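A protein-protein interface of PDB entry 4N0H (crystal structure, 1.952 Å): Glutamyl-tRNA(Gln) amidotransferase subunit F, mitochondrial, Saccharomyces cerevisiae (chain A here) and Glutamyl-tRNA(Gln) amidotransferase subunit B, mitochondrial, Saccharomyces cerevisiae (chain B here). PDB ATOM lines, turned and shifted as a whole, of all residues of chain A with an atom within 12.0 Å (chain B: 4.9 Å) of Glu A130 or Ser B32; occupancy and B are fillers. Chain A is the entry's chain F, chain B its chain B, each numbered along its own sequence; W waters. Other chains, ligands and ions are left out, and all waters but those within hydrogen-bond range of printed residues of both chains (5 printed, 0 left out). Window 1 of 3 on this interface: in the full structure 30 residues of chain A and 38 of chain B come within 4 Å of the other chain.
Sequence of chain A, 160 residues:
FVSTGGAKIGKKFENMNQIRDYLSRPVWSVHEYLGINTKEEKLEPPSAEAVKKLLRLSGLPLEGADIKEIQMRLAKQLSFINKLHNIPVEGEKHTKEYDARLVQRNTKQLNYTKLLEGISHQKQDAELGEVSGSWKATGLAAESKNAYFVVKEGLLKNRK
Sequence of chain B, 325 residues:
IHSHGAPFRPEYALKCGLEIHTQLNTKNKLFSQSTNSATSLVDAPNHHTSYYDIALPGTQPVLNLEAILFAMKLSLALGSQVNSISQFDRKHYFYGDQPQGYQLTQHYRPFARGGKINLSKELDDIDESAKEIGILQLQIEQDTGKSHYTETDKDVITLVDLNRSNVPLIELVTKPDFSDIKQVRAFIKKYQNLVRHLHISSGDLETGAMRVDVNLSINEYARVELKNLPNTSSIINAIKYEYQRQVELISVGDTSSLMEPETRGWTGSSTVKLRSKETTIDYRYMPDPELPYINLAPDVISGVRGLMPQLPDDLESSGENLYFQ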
ATOM      1  N   GLY A 118      13.708 -21.791  16.370  1.00  0.00           N
ATOM      2  CA  GLY A 118      12.266 -21.830  16.212  1.00  0.00           C
ATOM      3  C   GLY A 118      11.887 -22.378  14.849  1.00  0.00           C
ATOM      4  O   GLY A 118      11.030 -23.252  14.746  1.00  0.00           O
ATOM      5  N   ILE A 119      12.543 -21.869  13.808  1.00  0.00           N
ATOM      6  CA  ILE A 119      12.334 -22.339  12.443  1.00  0.00           C
ATOM      7  C   ILE A 119      12.601 -23.833  12.304  1.00  0.00           C
ATOM      8  O   ILE A 119      11.794 -24.563  11.728  1.00  0.00           O
ATOM      9  CB  ILE A 119      13.230 -21.575  11.438  1.00  0.00           C
ATOM     10  CG1 ILE A 119      12.753 -20.131  11.280  1.00  0.00           C
ATOM     11  CG2 ILE A 119      13.244 -22.263  10.079  1.00  0.00           C
ATOM     12  CD1 ILE A 119      13.591 -19.320  10.307  1.00  0.00           C
ATOM     13  N   HIS A 121      12.483 -26.169  14.432  1.00  0.00           N
ATOM     14  CA  HIS A 121      11.569 -27.013  15.197  1.00  0.00           C
ATOM     15  C   HIS A 121      10.111 -26.870  14.759  1.00  0.00           C
ATOM     16  O   HIS A 121       9.207 -27.366  15.427  1.00  0.00           O
ATOM     17  CB  HIS A 121      11.693 -26.720  16.692  1.00  0.00           C
ATOM     18  CG  HIS A 121      13.007 -27.131  17.279  1.00  0.00           C
ATOM     19  ND1 HIS A 121      13.261 -27.091  18.634  1.00  0.00           N
ATOM     20  CD2 HIS A 121      14.138 -27.593  16.696  1.00  0.00           C
ATOM     21  CE1 HIS A 121      14.495 -27.509  18.858  1.00  0.00           C
ATOM     22  NE2 HIS A 121      15.048 -27.819  17.700  1.00  0.00           N
ATOM     23  N   GLN A 122       9.884 -26.185  13.643  1.00  0.00           N
ATOM     24  CA  GLN A 122       8.532 -26.054  13.107  1.00  0.00           C
ATOM     25  C   GLN A 122       8.160 -27.303  12.318  1.00  0.00           C
ATOM     26  O   GLN A 122       8.953 -27.803  11.524  1.00  0.00           O
ATOM     27  CB  GLN A 122       8.408 -24.802  12.238  1.00  0.00           C
ATOM     28  CG  GLN A 122       8.462 -23.510  13.040  1.00  0.00           C
ATOM     29  CD  GLN A 122       8.264 -22.267  12.188  1.00  0.00           C
ATOM     30  OE1 GLN A 122       7.834 -21.221  12.687  1.00  0.00           O
ATOM     31  NE2 GLN A 122       8.579 -22.373  10.892  1.00  0.00           N
ATOM     32  N   LYS A 123       6.960 -27.818  12.558  1.00  0.00           N
ATOM     33  CA  LYS A 123       6.517 -29.041  11.901  1.00  0.00           C
ATOM     34  C   LYS A 123       4.998 -29.094  11.839  1.00  0.00           C
ATOM     35  O   LYS A 123       4.310 -28.336  12.522  1.00  0.00           O
ATOM     36  CB  LYS A 123       7.057 -30.267  12.639  1.00  0.00           C
ATOM     37  CG  LYS A 123       6.438 -30.480  14.008  1.00  0.00           C
ATOM     38  CD  LYS A 123       7.344 -31.304  14.906  1.00  0.00           C
ATOM     39  CE  LYS A 123       8.611 -30.534  15.240  1.00  0.00           C
ATOM     40  NZ  LYS A 123       9.460 -31.245  16.232  1.00  0.00           N
ATOM     41  N   GLN A 124       4.479 -29.995  11.014  1.00  0.00           N
ATOM     42  CA  GLN A 124       3.039 -30.159  10.881  1.00  0.00           C
ATOM     43  C   GLN A 124       2.491 -31.022  12.018  1.00  0.00           C
ATOM     44  O   GLN A 124       2.968 -32.128  12.264  1.00  0.00           O
ATOM     45  CB  GLN A 124       2.689 -30.739   9.512  1.00  0.00           C
ATOM     46  CG  GLN A 124       3.277 -29.916   8.365  1.00  0.00           C
ATOM     47  CD  GLN A 124       2.742 -30.329   7.010  1.00  0.00           C
ATOM     48  OE1 GLN A 124       2.735 -31.513   6.669  1.00  0.00           O
ATOM     49  NE2 GLN A 124       2.286 -29.351   6.231  1.00  0.00           N
ATOM     50  N   ASP A 125       1.494 -30.485  12.711  1.00  0.00           N
ATOM     51  CA  ASP A 125       0.913 -31.117  13.888  1.00  0.00           C
ATOM     52  C   ASP A 125      -0.405 -31.777  13.513  1.00  0.00           C
ATOM     53  O   ASP A 125      -1.334 -31.111  13.054  1.00  0.00           O
ATOM     54  CB  ASP A 125       0.670 -30.048  14.963  1.00  0.00           C
ATOM     55  CG  ASP A 125       0.301 -30.633  16.320  1.00  0.00           C
ATOM     56  OD1 ASP A 125      -0.001 -31.842  16.409  1.00  0.00           O
ATOM     57  OD2 ASP A 125       0.305 -29.860  17.306  1.00  0.00           O
ATOM     58  N   ALA A 126      -0.487 -33.084  13.727  1.00  0.00           N
ATOM     59  CA  ALA A 126      -1.712 -33.836  13.474  1.00  0.00           C
ATOM     60  C   ALA A 126      -2.893 -33.271  14.260  1.00  0.00           C
ATOM     61  O   ALA A 126      -4.027 -33.269  13.780  1.00  0.00           O
ATOM     62  CB  ALA A 126      -1.507 -35.307  13.821  1.00  0.00           C
ATOM     63  N   GLU A 127      -2.619 -32.775  15.463  1.00  0.00           N
ATOM     64  CA  GLU A 127      -3.676 -32.245  16.318  1.00  0.00           C
ATOM     65  C   GLU A 127      -4.206 -30.899  15.824  1.00  0.00           C
ATOM     66  O   GLU A 127      -5.191 -30.384  16.347  1.00  0.00           O
ATOM     67  CB  GLU A 127      -3.188 -32.130  17.765  1.00  0.00           C
ATOM     68  CG  GLU A 127      -2.854 -33.463  18.422  1.00  0.00           C
ATOM     69  CD  GLU A 127      -2.494 -33.318  19.891  1.00  0.00           C
ATOM     70  OE1 GLU A 127      -2.015 -32.234  20.288  1.00  0.00           O
ATOM     71  OE2 GLU A 127      -2.694 -34.289  20.652  1.00  0.00           O
ATOM     72  N   LEU A 128      -3.546 -30.334  14.816  1.00  0.00           N
ATOM     73  CA  LEU A 128      -3.991 -29.089  14.194  1.00  0.00           C
ATOM     74  C   LEU A 128      -4.523 -29.323  12.779  1.00  0.00           C
ATOM     75  O   LEU A 128      -4.993 -28.390  12.128  1.00  0.00           O
ATOM     76  CB  LEU A 128      -2.846 -28.073  14.151  1.00  0.00           C
ATOM     77  CG  LEU A 128      -2.339 -27.543  15.496  1.00  0.00           C
ATOM     78  CD1 LEU A 128      -1.111 -26.661  15.307  1.00  0.00           C
ATOM     79  CD2 LEU A 128      -3.445 -26.776  16.196  1.00  0.00           C
ATOM     80  N   GLY A 129      -4.451 -30.569  12.313  1.00  0.00           N
ATOM     81  CA  GLY A 129      -4.919 -30.925  10.982  1.00  0.00           C
ATOM     82  C   GLY A 129      -4.025 -30.360   9.890  1.00  0.00           C
ATOM     83  O   GLY A 129      -4.483 -30.041   8.795  1.00  0.00           O
ATOM     84  N   GLU A 130      -2.736 -30.243  10.190  1.00  0.00           N
ATOM     85  CA  GLU A 130      -1.815 -29.532   9.310  1.00  0.00           C
ATOM     86  C   GLU A 130      -1.221 -30.405   8.199  1.00  0.00           C
ATOM     87  O   GLU A 130      -0.688 -29.884   7.225  1.00  0.00           O
ATOM     88  CB  GLU A 130      -0.711 -28.852  10.130  1.00  0.00           C
ATOM     89  CG  GLU A 130      -1.182 -27.563  10.808  1.00  0.00           C
ATOM     90  CD  GLU A 130      -0.210 -27.045  11.849  1.00  0.00           C
ATOM     91  OE1 GLU A 130       0.611 -27.842  12.350  1.00  0.00           O
ATOM     92  OE2 GLU A 130      -0.265 -25.836  12.166  1.00  0.00           O
ATOM     93  N   VAL A 131      -1.311 -31.725   8.339  1.00  0.00           N
ATOM     94  CA  VAL A 131      -0.835 -32.606   7.274  1.00  0.00           C
ATOM     95  C   VAL A 131      -1.868 -32.621   6.157  1.00  0.00           C
ATOM     96  O   VAL A 131      -3.051 -32.850   6.404  1.00  0.00           O
ATOM     97  CB  VAL A 131      -0.594 -34.040   7.765  1.00  0.00           C
ATOM     98  CG1 VAL A 131      -0.069 -34.909   6.624  1.00  0.00           C
ATOM     99  CG2 VAL A 131       0.376 -34.047   8.929  1.00  0.00           C
ATOM    100  N   SER A 132      -1.419 -32.354   4.936  1.00  0.00           N
ATOM    101  CA  SER A 132      -2.298 -32.315   3.770  1.00  0.00           C
ATOM    102  C   SER A 132      -3.150 -33.574   3.651  1.00  0.00           C
ATOM    103  O   SER A 132      -2.638 -34.690   3.731  1.00  0.00           O
ATOM    104  CB  SER A 132      -1.476 -32.136   2.489  1.00  0.00           C
ATOM    105  OG  SER A 132      -0.787 -30.899   2.485  1.00  0.00           O
ATOM    106  N   GLY A 133      -4.452 -33.382   3.471  1.00  0.00           N
ATOM    107  CA  GLY A 133      -5.384 -34.482   3.294  1.00  0.00           C
ATOM    108  C   GLY A 133      -5.661 -35.326   4.524  1.00  0.00           C
ATOM    109  O   GLY A 133      -6.253 -36.399   4.417  1.00  0.00           O
ATOM    110  N   SER A 134      -5.253 -34.850   5.697  1.00  0.00           N
ATOM    111  CA  SER A 134      -5.413 -35.630   6.921  1.00  0.00           C
ATOM    112  C   SER A 134      -6.847 -35.617   7.443  1.00  0.00           C
ATOM    113  O   SER A 134      -7.203 -36.408   8.315  1.00  0.00           O
ATOM    114  CB  SER A 134      -4.458 -35.139   8.010  1.00  0.00           C
ATOM    115  OG  SER A 134      -4.809 -33.838   8.450  1.00  0.00           O
ATOM    116  N   TRP A 135      -7.662 -34.709   6.916  1.00  0.00           N
ATOM    117  CA  TRP A 135      -9.073 -34.647   7.274  1.00  0.00           C
ATOM    118  C   TRP A 135      -9.865 -34.085   6.100  1.00  0.00           C
ATOM    119  O   TRP A 135      -9.288 -33.495   5.191  1.00  0.00           O
ATOM    120  CB  TRP A 135      -9.281 -33.798   8.533  1.00  0.00           C
ATOM    121  CG  TRP A 135      -8.986 -32.335   8.348  1.00  0.00           C
ATOM    122  CD1 TRP A 135      -7.769 -31.766   8.087  1.00  0.00           C
ATOM    123  CD2 TRP A 135      -9.926 -31.255   8.411  1.00  0.00           C
ATOM    124  NE1 TRP A 135      -7.896 -30.402   7.984  1.00  0.00           N
ATOM    125  CE2 TRP A 135      -9.211 -30.062   8.179  1.00  0.00           C
ATOM    126  CE3 TRP A 135     -11.304 -31.181   8.645  1.00  0.00           C
ATOM    127  CZ2 TRP A 135      -9.825 -28.810   8.172  1.00  0.00           C
ATOM    128  CZ3 TRP A 135     -11.912 -29.940   8.636  1.00  0.00           C
ATOM    129  CH2 TRP A 135     -11.173 -28.770   8.401  1.00  0.00           C
ATOM    130  N   LYS A 136     -11.180 -34.279   6.109  1.00  0.00           N
ATOM    131  CA  LYS A 136     -12.020 -33.769   5.029  1.00  0.00           C
ATOM    132  C   LYS A 136     -12.424 -32.325   5.308  1.00  0.00           C
ATOM    133  O   LYS A 136     -13.381 -32.063   6.041  1.00  0.00           O
ATOM    134  CB  LYS A 136     -13.259 -34.648   4.829  1.00  0.00           C
ATOM    135  CG  LYS A 136     -13.563 -34.934   3.366  1.00  0.00           C
ATOM    136  CD  LYS A 136     -14.897 -34.346   2.921  1.00  0.00           C
ATOM    137  CE  LYS A 136     -16.018 -35.377   3.003  1.00  0.00           C
ATOM    138  NZ  LYS A 136     -17.323 -34.847   2.501  1.00  0.00           N
ATOM    139  N   ALA A 137     -11.680 -31.396   4.716  1.00  0.00           N
ATOM    140  CA  ALA A 137     -11.853 -29.973   4.981  1.00  0.00           C
ATOM    141  C   ALA A 137     -13.235 -29.451   4.602  1.00  0.00           C
ATOM    142  O   ALA A 137     -13.708 -28.469   5.172  1.00  0.00           O
ATOM    143  CB  ALA A 137     -10.766 -29.173   4.276  1.00  0.00           C
ATOM    144  N   ASN B  28       5.793 -23.844   4.582  1.00  0.00           N
ATOM    145  CA  ASN B  28       4.434 -23.863   5.104  1.00  0.00           C
ATOM    146  C   ASN B  28       3.822 -22.469   5.132  1.00  0.00           C
ATOM    147  O   ASN B  28       4.479 -21.501   4.760  1.00  0.00           O
ATOM    148  CB  ASN B  28       4.413 -24.523   6.485  1.00  0.00           C
ATOM    149  CG  ASN B  28       4.892 -25.965   6.434  1.00  0.00           C
ATOM    150  OD1 ASN B  28       4.665 -26.668   5.444  1.00  0.00           O
ATOM    151  ND2 ASN B  28       5.570 -26.407   7.486  1.00  0.00           N
ATOM    152  N   LYS B  29       2.566 -22.374   5.558  1.00  0.00           N
ATOM    153  CA  LYS B  29       1.818 -21.126   5.470  1.00  0.00           C
ATOM    154  C   LYS B  29       2.169 -20.135   6.577  1.00  0.00           C
ATOM    155  O   LYS B  29       3.037 -20.401   7.397  1.00  0.00           O
ATOM    156  CB  LYS B  29       0.320 -21.400   5.464  1.00  0.00           C
ATOM    157  CG  LYS B  29      -0.160 -22.171   4.243  1.00  0.00           C
ATOM    158  CD  LYS B  29      -1.683 -22.179   4.217  1.00  0.00           C
ATOM    159  CE  LYS B  29      -2.233 -23.100   3.150  1.00  0.00           C
ATOM    160  NZ  LYS B  29      -3.721 -22.990   3.125  1.00  0.00           N
ATOM    161  N   LEU B  30       1.484 -18.997   6.586  1.00  0.00           N
ATOM    162  CA  LEU B  30       1.846 -17.873   7.457  1.00  0.00           C
ATOM    163  C   LEU B  30       1.470 -18.058   8.939  1.00  0.00           C
ATOM    164  O   LEU B  30       2.312 -17.902   9.827  1.00  0.00           O
ATOM    165  CB  LEU B  30       1.242 -16.571   6.916  1.00  0.00           C
ATOM    166  CG  LEU B  30       1.639 -15.292   7.652  1.00  0.00           C
ATOM    167  CD1 LEU B  30       3.158 -15.181   7.727  1.00  0.00           C
ATOM    168  CD2 LEU B  30       1.053 -14.060   6.969  1.00  0.00           C
ATOM    169  N   PHE B  31       0.211 -18.385   9.206  1.00  0.00           N
ATOM    170  CA  PHE B  31      -0.243 -18.549  10.588  1.00  0.00           C
ATOM    171  C   PHE B  31      -0.675 -19.982  10.908  1.00  0.00           C
ATOM    172  O   PHE B  31      -1.373 -20.232  11.886  1.00  0.00           O
ATOM    173  CB  PHE B  31      -1.363 -17.551  10.902  1.00  0.00           C
ATOM    174  CG  PHE B  31      -0.901 -16.126  10.908  1.00  0.00           C
ATOM    175  CD1 PHE B  31      -0.100 -15.652  11.937  1.00  0.00           C
ATOM    176  CD2 PHE B  31      -1.233 -15.267   9.873  1.00  0.00           C
ATOM    177  CE1 PHE B  31       0.342 -14.342  11.944  1.00  0.00           C
ATOM    178  CE2 PHE B  31      -0.794 -13.956   9.874  1.00  0.00           C
ATOM    179  CZ  PHE B  31       0.002 -13.494  10.906  1.00  0.00           C
ATOM    180  N   SER B  32      -0.260 -20.913  10.059  1.00  0.00           N
ATOM    181  CA  SER B  32      -0.511 -22.332  10.259  1.00  0.00           C
ATOM    182  C   SER B  32       0.625 -23.089   9.589  1.00  0.00           C
ATOM    183  O   SER B  32       1.235 -22.584   8.646  1.00  0.00           O
ATOM    184  CB  SER B  32      -1.845 -22.734   9.627  1.00  0.00           C
ATOM    185  OG  SER B  32      -2.028 -24.139   9.669  1.00  0.00           O
ATOM    186  N   GLN B  33       0.915 -24.296  10.061  1.00  0.00           N
ATOM    187  CA  GLN B  33       2.004 -25.070   9.468  1.00  0.00           C
ATOM    188  C   GLN B  33       1.551 -25.981   8.323  1.00  0.00           C
ATOM    189  O   GLN B  33       2.283 -26.879   7.904  1.00  0.00           O
ATOM    190  CB  GLN B  33       2.776 -25.853  10.536  1.00  0.00           C
ATOM    191  CG  GLN B  33       3.686 -24.974  11.388  1.00  0.00           C
ATOM    192  CD  GLN B  33       4.699 -24.207  10.545  1.00  0.00           C
ATOM    193  OE1 GLN B  33       5.524 -24.801   9.847  1.00  0.00           O
ATOM    194  NE2 GLN B  33       4.632 -22.885  10.597  1.00  0.00           N
ATOM    195  N   SER B  34       0.347 -25.742   7.816  1.00  0.00           N
ATOM    196  CA  SER B  34      -0.123 -26.444   6.627  1.00  0.00           C
ATOM    197  C   SER B  34       0.750 -26.088   5.426  1.00  0.00           C
ATOM    198  O   SER B  34       1.427 -25.055   5.412  1.00  0.00           O
ATOM    199  CB  SER B  34      -1.593 -26.111   6.349  1.00  0.00           C
ATOM    200  OG  SER B  34      -1.818 -24.711   6.445  1.00  0.00           O
ATOM    201  N   THR B  35       0.730 -26.947   4.414  1.00  0.00           N
ATOM    202  CA  THR B  35       1.640 -26.822   3.288  1.00  0.00           C
ATOM    203  C   THR B  35       1.369 -25.598   2.418  1.00  0.00           C
ATOM    204  O   THR B  35       0.228 -25.319   2.050  1.00  0.00           O
ATOM    205  CB  THR B  35       1.596 -28.094   2.411  1.00  0.00           C
ATOM    206  OG1 THR B  35       1.979 -29.225   3.205  1.00  0.00           O
ATOM    207  CG2 THR B  35       2.532 -27.967   1.210  1.00  0.00           C
ATOM    208  N   SER B  50      -5.421 -26.654   7.116  1.00  0.00           N
ATOM    209  CA  SER B  50      -5.536 -27.025   8.522  1.00  0.00           C
ATOM    210  C   SER B  50      -6.897 -26.637   9.087  1.00  0.00           C
ATOM    211  O   SER B  50      -7.704 -26.002   8.406  1.00  0.00           O
ATOM    212  CB  SER B  50      -4.446 -26.316   9.321  1.00  0.00           C
ATOM    213  OG  SER B  50      -4.551 -24.912   9.125  1.00  0.00           O
ATOM    214  N   TYR B  52      -7.200 -24.414  11.246  1.00  0.00           N
ATOM    215  CA  TYR B  52      -7.118 -22.953  11.251  1.00  0.00           C
ATOM    216  C   TYR B  52      -7.439 -22.342   9.887  1.00  0.00           C
ATOM    217  O   TYR B  52      -8.113 -21.316   9.814  1.00  0.00           O
ATOM    218  CB  TYR B  52      -5.740 -22.465  11.714  1.00  0.00           C
ATOM    219  CG  TYR B  52      -5.552 -20.976  11.520  1.00  0.00           C
ATOM    220  CD1 TYR B  52      -6.049 -20.067  12.445  1.00  0.00           C
ATOM    221  CD2 TYR B  52      -4.896 -20.481  10.398  1.00  0.00           C
ATOM    222  CE1 TYR B  52      -5.894 -18.699  12.259  1.00  0.00           C
ATOM    223  CE2 TYR B  52      -4.740 -19.123  10.201  1.00  0.00           C
ATOM    224  CZ  TYR B  52      -5.233 -18.239  11.136  1.00  0.00           C
ATOM    225  OH  TYR B  52      -5.065 -16.889  10.934  1.00  0.00           O
ATOM    226  N   ASP B  53      -6.945 -22.959   8.816  1.00  0.00           N
ATOM    227  CA  ASP B  53      -7.173 -22.437   7.466  1.00  0.00           C
ATOM    228  C   ASP B  53      -8.670 -22.378   7.138  1.00  0.00           C
ATOM    229  O   ASP B  53      -9.118 -21.515   6.386  1.00  0.00           O
ATOM    230  CB  ASP B  53      -6.448 -23.284   6.414  1.00  0.00           C
ATOM    231  CG  ASP B  53      -4.935 -23.177   6.507  1.00  0.00           C
ATOM    232  OD1 ASP B  53      -4.427 -22.206   7.109  1.00  0.00           O
ATOM    233  OD2 ASP B  53      -4.250 -24.073   5.971  1.00  0.00           O
ATOM    234  N   VAL B  62      -0.695 -19.062  14.644  1.00  0.00           N
ATOM    235  CA  VAL B  62       0.673 -19.107  15.170  1.00  0.00           C
ATOM    236  C   VAL B  62       1.641 -18.700  14.056  1.00  0.00           C
ATOM    237  O   VAL B  62       1.675 -19.327  12.992  1.00  0.00           O
ATOM    238  CB  VAL B  62       1.058 -20.508  15.686  1.00  0.00           C
ATOM    239  CG1 VAL B  62       2.514 -20.529  16.131  1.00  0.00           C
ATOM    240  CG2 VAL B  62       0.136 -20.943  16.830  1.00  0.00           C
ATOM    241  N   ASN B 166      -4.156 -18.079   3.637  1.00  0.00           N
ATOM    242  CA  ASN B 166      -3.133 -18.108   4.684  1.00  0.00           C
ATOM    243  C   ASN B 166      -1.705 -18.330   4.155  1.00  0.00           C
ATOM    244  O   ASN B 166      -0.764 -18.507   4.927  1.00  0.00           O
ATOM    245  CB  ASN B 166      -3.513 -19.119   5.778  1.00  0.00           C
ATOM    246  CG  ASN B 166      -2.676 -18.976   7.023  1.00  0.00           C
ATOM    247  OD1 ASN B 166      -2.288 -17.873   7.403  1.00  0.00           O
ATOM    248  ND2 ASN B 166      -2.389 -20.098   7.665  1.00  0.00           N
HETATM  249  O   HOH W   1       1.367 -32.125   4.413  1.00  0.00           O
HETATM  250  O   HOH W   2       8.271 -24.248   8.869  1.00  0.00           O
HETATM  251  O   HOH W   3      -1.011 -29.041   4.646  1.00  0.00           O
HETATM  252  O   HOH W   4      -5.125 -25.618  12.858  1.00  0.00           O
HETATM  253  O   HOH W   5      -2.601 -24.559  12.349  1.00  0.00           O
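Of the 19 printed residues of chain A, 8 touch a printed residue of chain B.
Of the 13 printed residues of chain B, 6 touch a printed residue of chain A.
Among the printed residues, 14 pairs touch across the chains.
Ser B32 touches just one residue of chain A: Glu A130 (3.5 Å).
No residue of chain A comes within 4 Å of Lys B29.
Of chain A, only Gln A122, Lys A123, Gln A124 and Glu A130 come within 4 Å of Gln B33.
Of chain A, only Gln A124 and Ser A132 come within 4 Å of Thr B35.
Of chain A, only Leu A128 (3.5 Å), Gly A129 (3.2 Å), Glu A130 (3.8 Å) and Trp A135 (3.5 Å) come within 4 Å of Ser B50.
No residue of chain A comes within 4 Å of Val B62.
Of the printed residues of chain B, Leu A128 touches Ser B50.
Of the printed residues of chain B, Ser A132 touches Thr B35.
Printed residues of chain B within 4 Å of Gln A124: Asn B28 (3.7 Å), Gln B33 (3.0 Å), Ser B34 (3.7 Å) and Thr B35 (3.0 Å).
Of the printed residues of chain B, Trp A135 touches Ser B50 (3.5 Å).
Asp A125 touches none of the printed residues of chain B.
The nearest residue of chain B that does not touch Glu A130 is Thr B35 (4.3 Å).
The side-chain hydroxyl of Ser B32 is in hydrogen-bond range of the side-chain hydroxyl of Ser B34 (3.3 Å).
The side-chain amide nitrogen (ND2) of Asn B166 sits close to the backbone NH (N) of Ser B32 (3.3 Å).
The side-chain carboxylate (OD2) of Asp B53 sits at hydrogen-bond distance from the side-chain hydroxyl (OG) of Ser B34 (2.6 Å).
OG of Ser B50 lies close to N of Tyr B52.
The side-chain amide nitrogen (NE2) of Gln A124 sits at hydrogen-bond distance from the backbone carbonyl oxygen (O) of Glu A130 (3.2 Å).
The backbone NH of Asp A125 is in hydrogen-bond range of the side-chain carboxylate of Glu A130, 2.8 Å away.
Among the printed residues, pairs that only touch across the chains: Gly A129 with Ser B50 (3.2 Å), Trp A135 with Ser B50 (3.5 Å), Lys A123 with Gln B33 (3.5 Å), Leu A128 with Ser B50 (3.5 Å), Glu A130 with Ser B34 (3.5 Å), Gln A124 with Asn B28 (3.7 Å), Gln A124 with Ser B34 (3.7 Å), Gln A122 with Gln B33 (3.7 Å) and Glu A130 with Ser B50 (3.8 Å).
Water W5 bridges the side-chain carboxylate of Glu A130 (2.7 Å) and the side-chain hydroxyl of Ser B32 (2.8 Å).
Water W1 lies within hydrogen-bond range of OE1 of Gln A124, N of Ser A132 and OG1 of Thr B35.
Water W3 lies within hydrogen-bond range of O of Glu A130 (2.7 Å), N of Thr B35 (2.7 Å) and OG of Ser A132 (2.9 Å).
Water W2 lies within hydrogen-bond range of NE2 of Gln A122 (2.8 Å) and OE1 of Gln B33 (3.0 Å).
Water W4 bridges O of Leu A128 and N of Tyr B52.
OG of Ser B32 is in hydrogen-bond range of OE2 of Glu A130.
O of Gln B33 lies within hydrogen-bond range of NE2 of Gln A124.
The backbone NH of Gln B33 sits at hydrogen-bond distance from the side-chain carboxylate of Glu A130 (2.9 Å).
The side-chain hydroxyl (OG1) of Thr B35 is in hydrogen-bond range of the side-chain amide nitrogen (NE2) of Gln A124, at 3.0 Å.
OG1 of Thr B35 sits at hydrogen-bond distance from OG of Ser A132.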
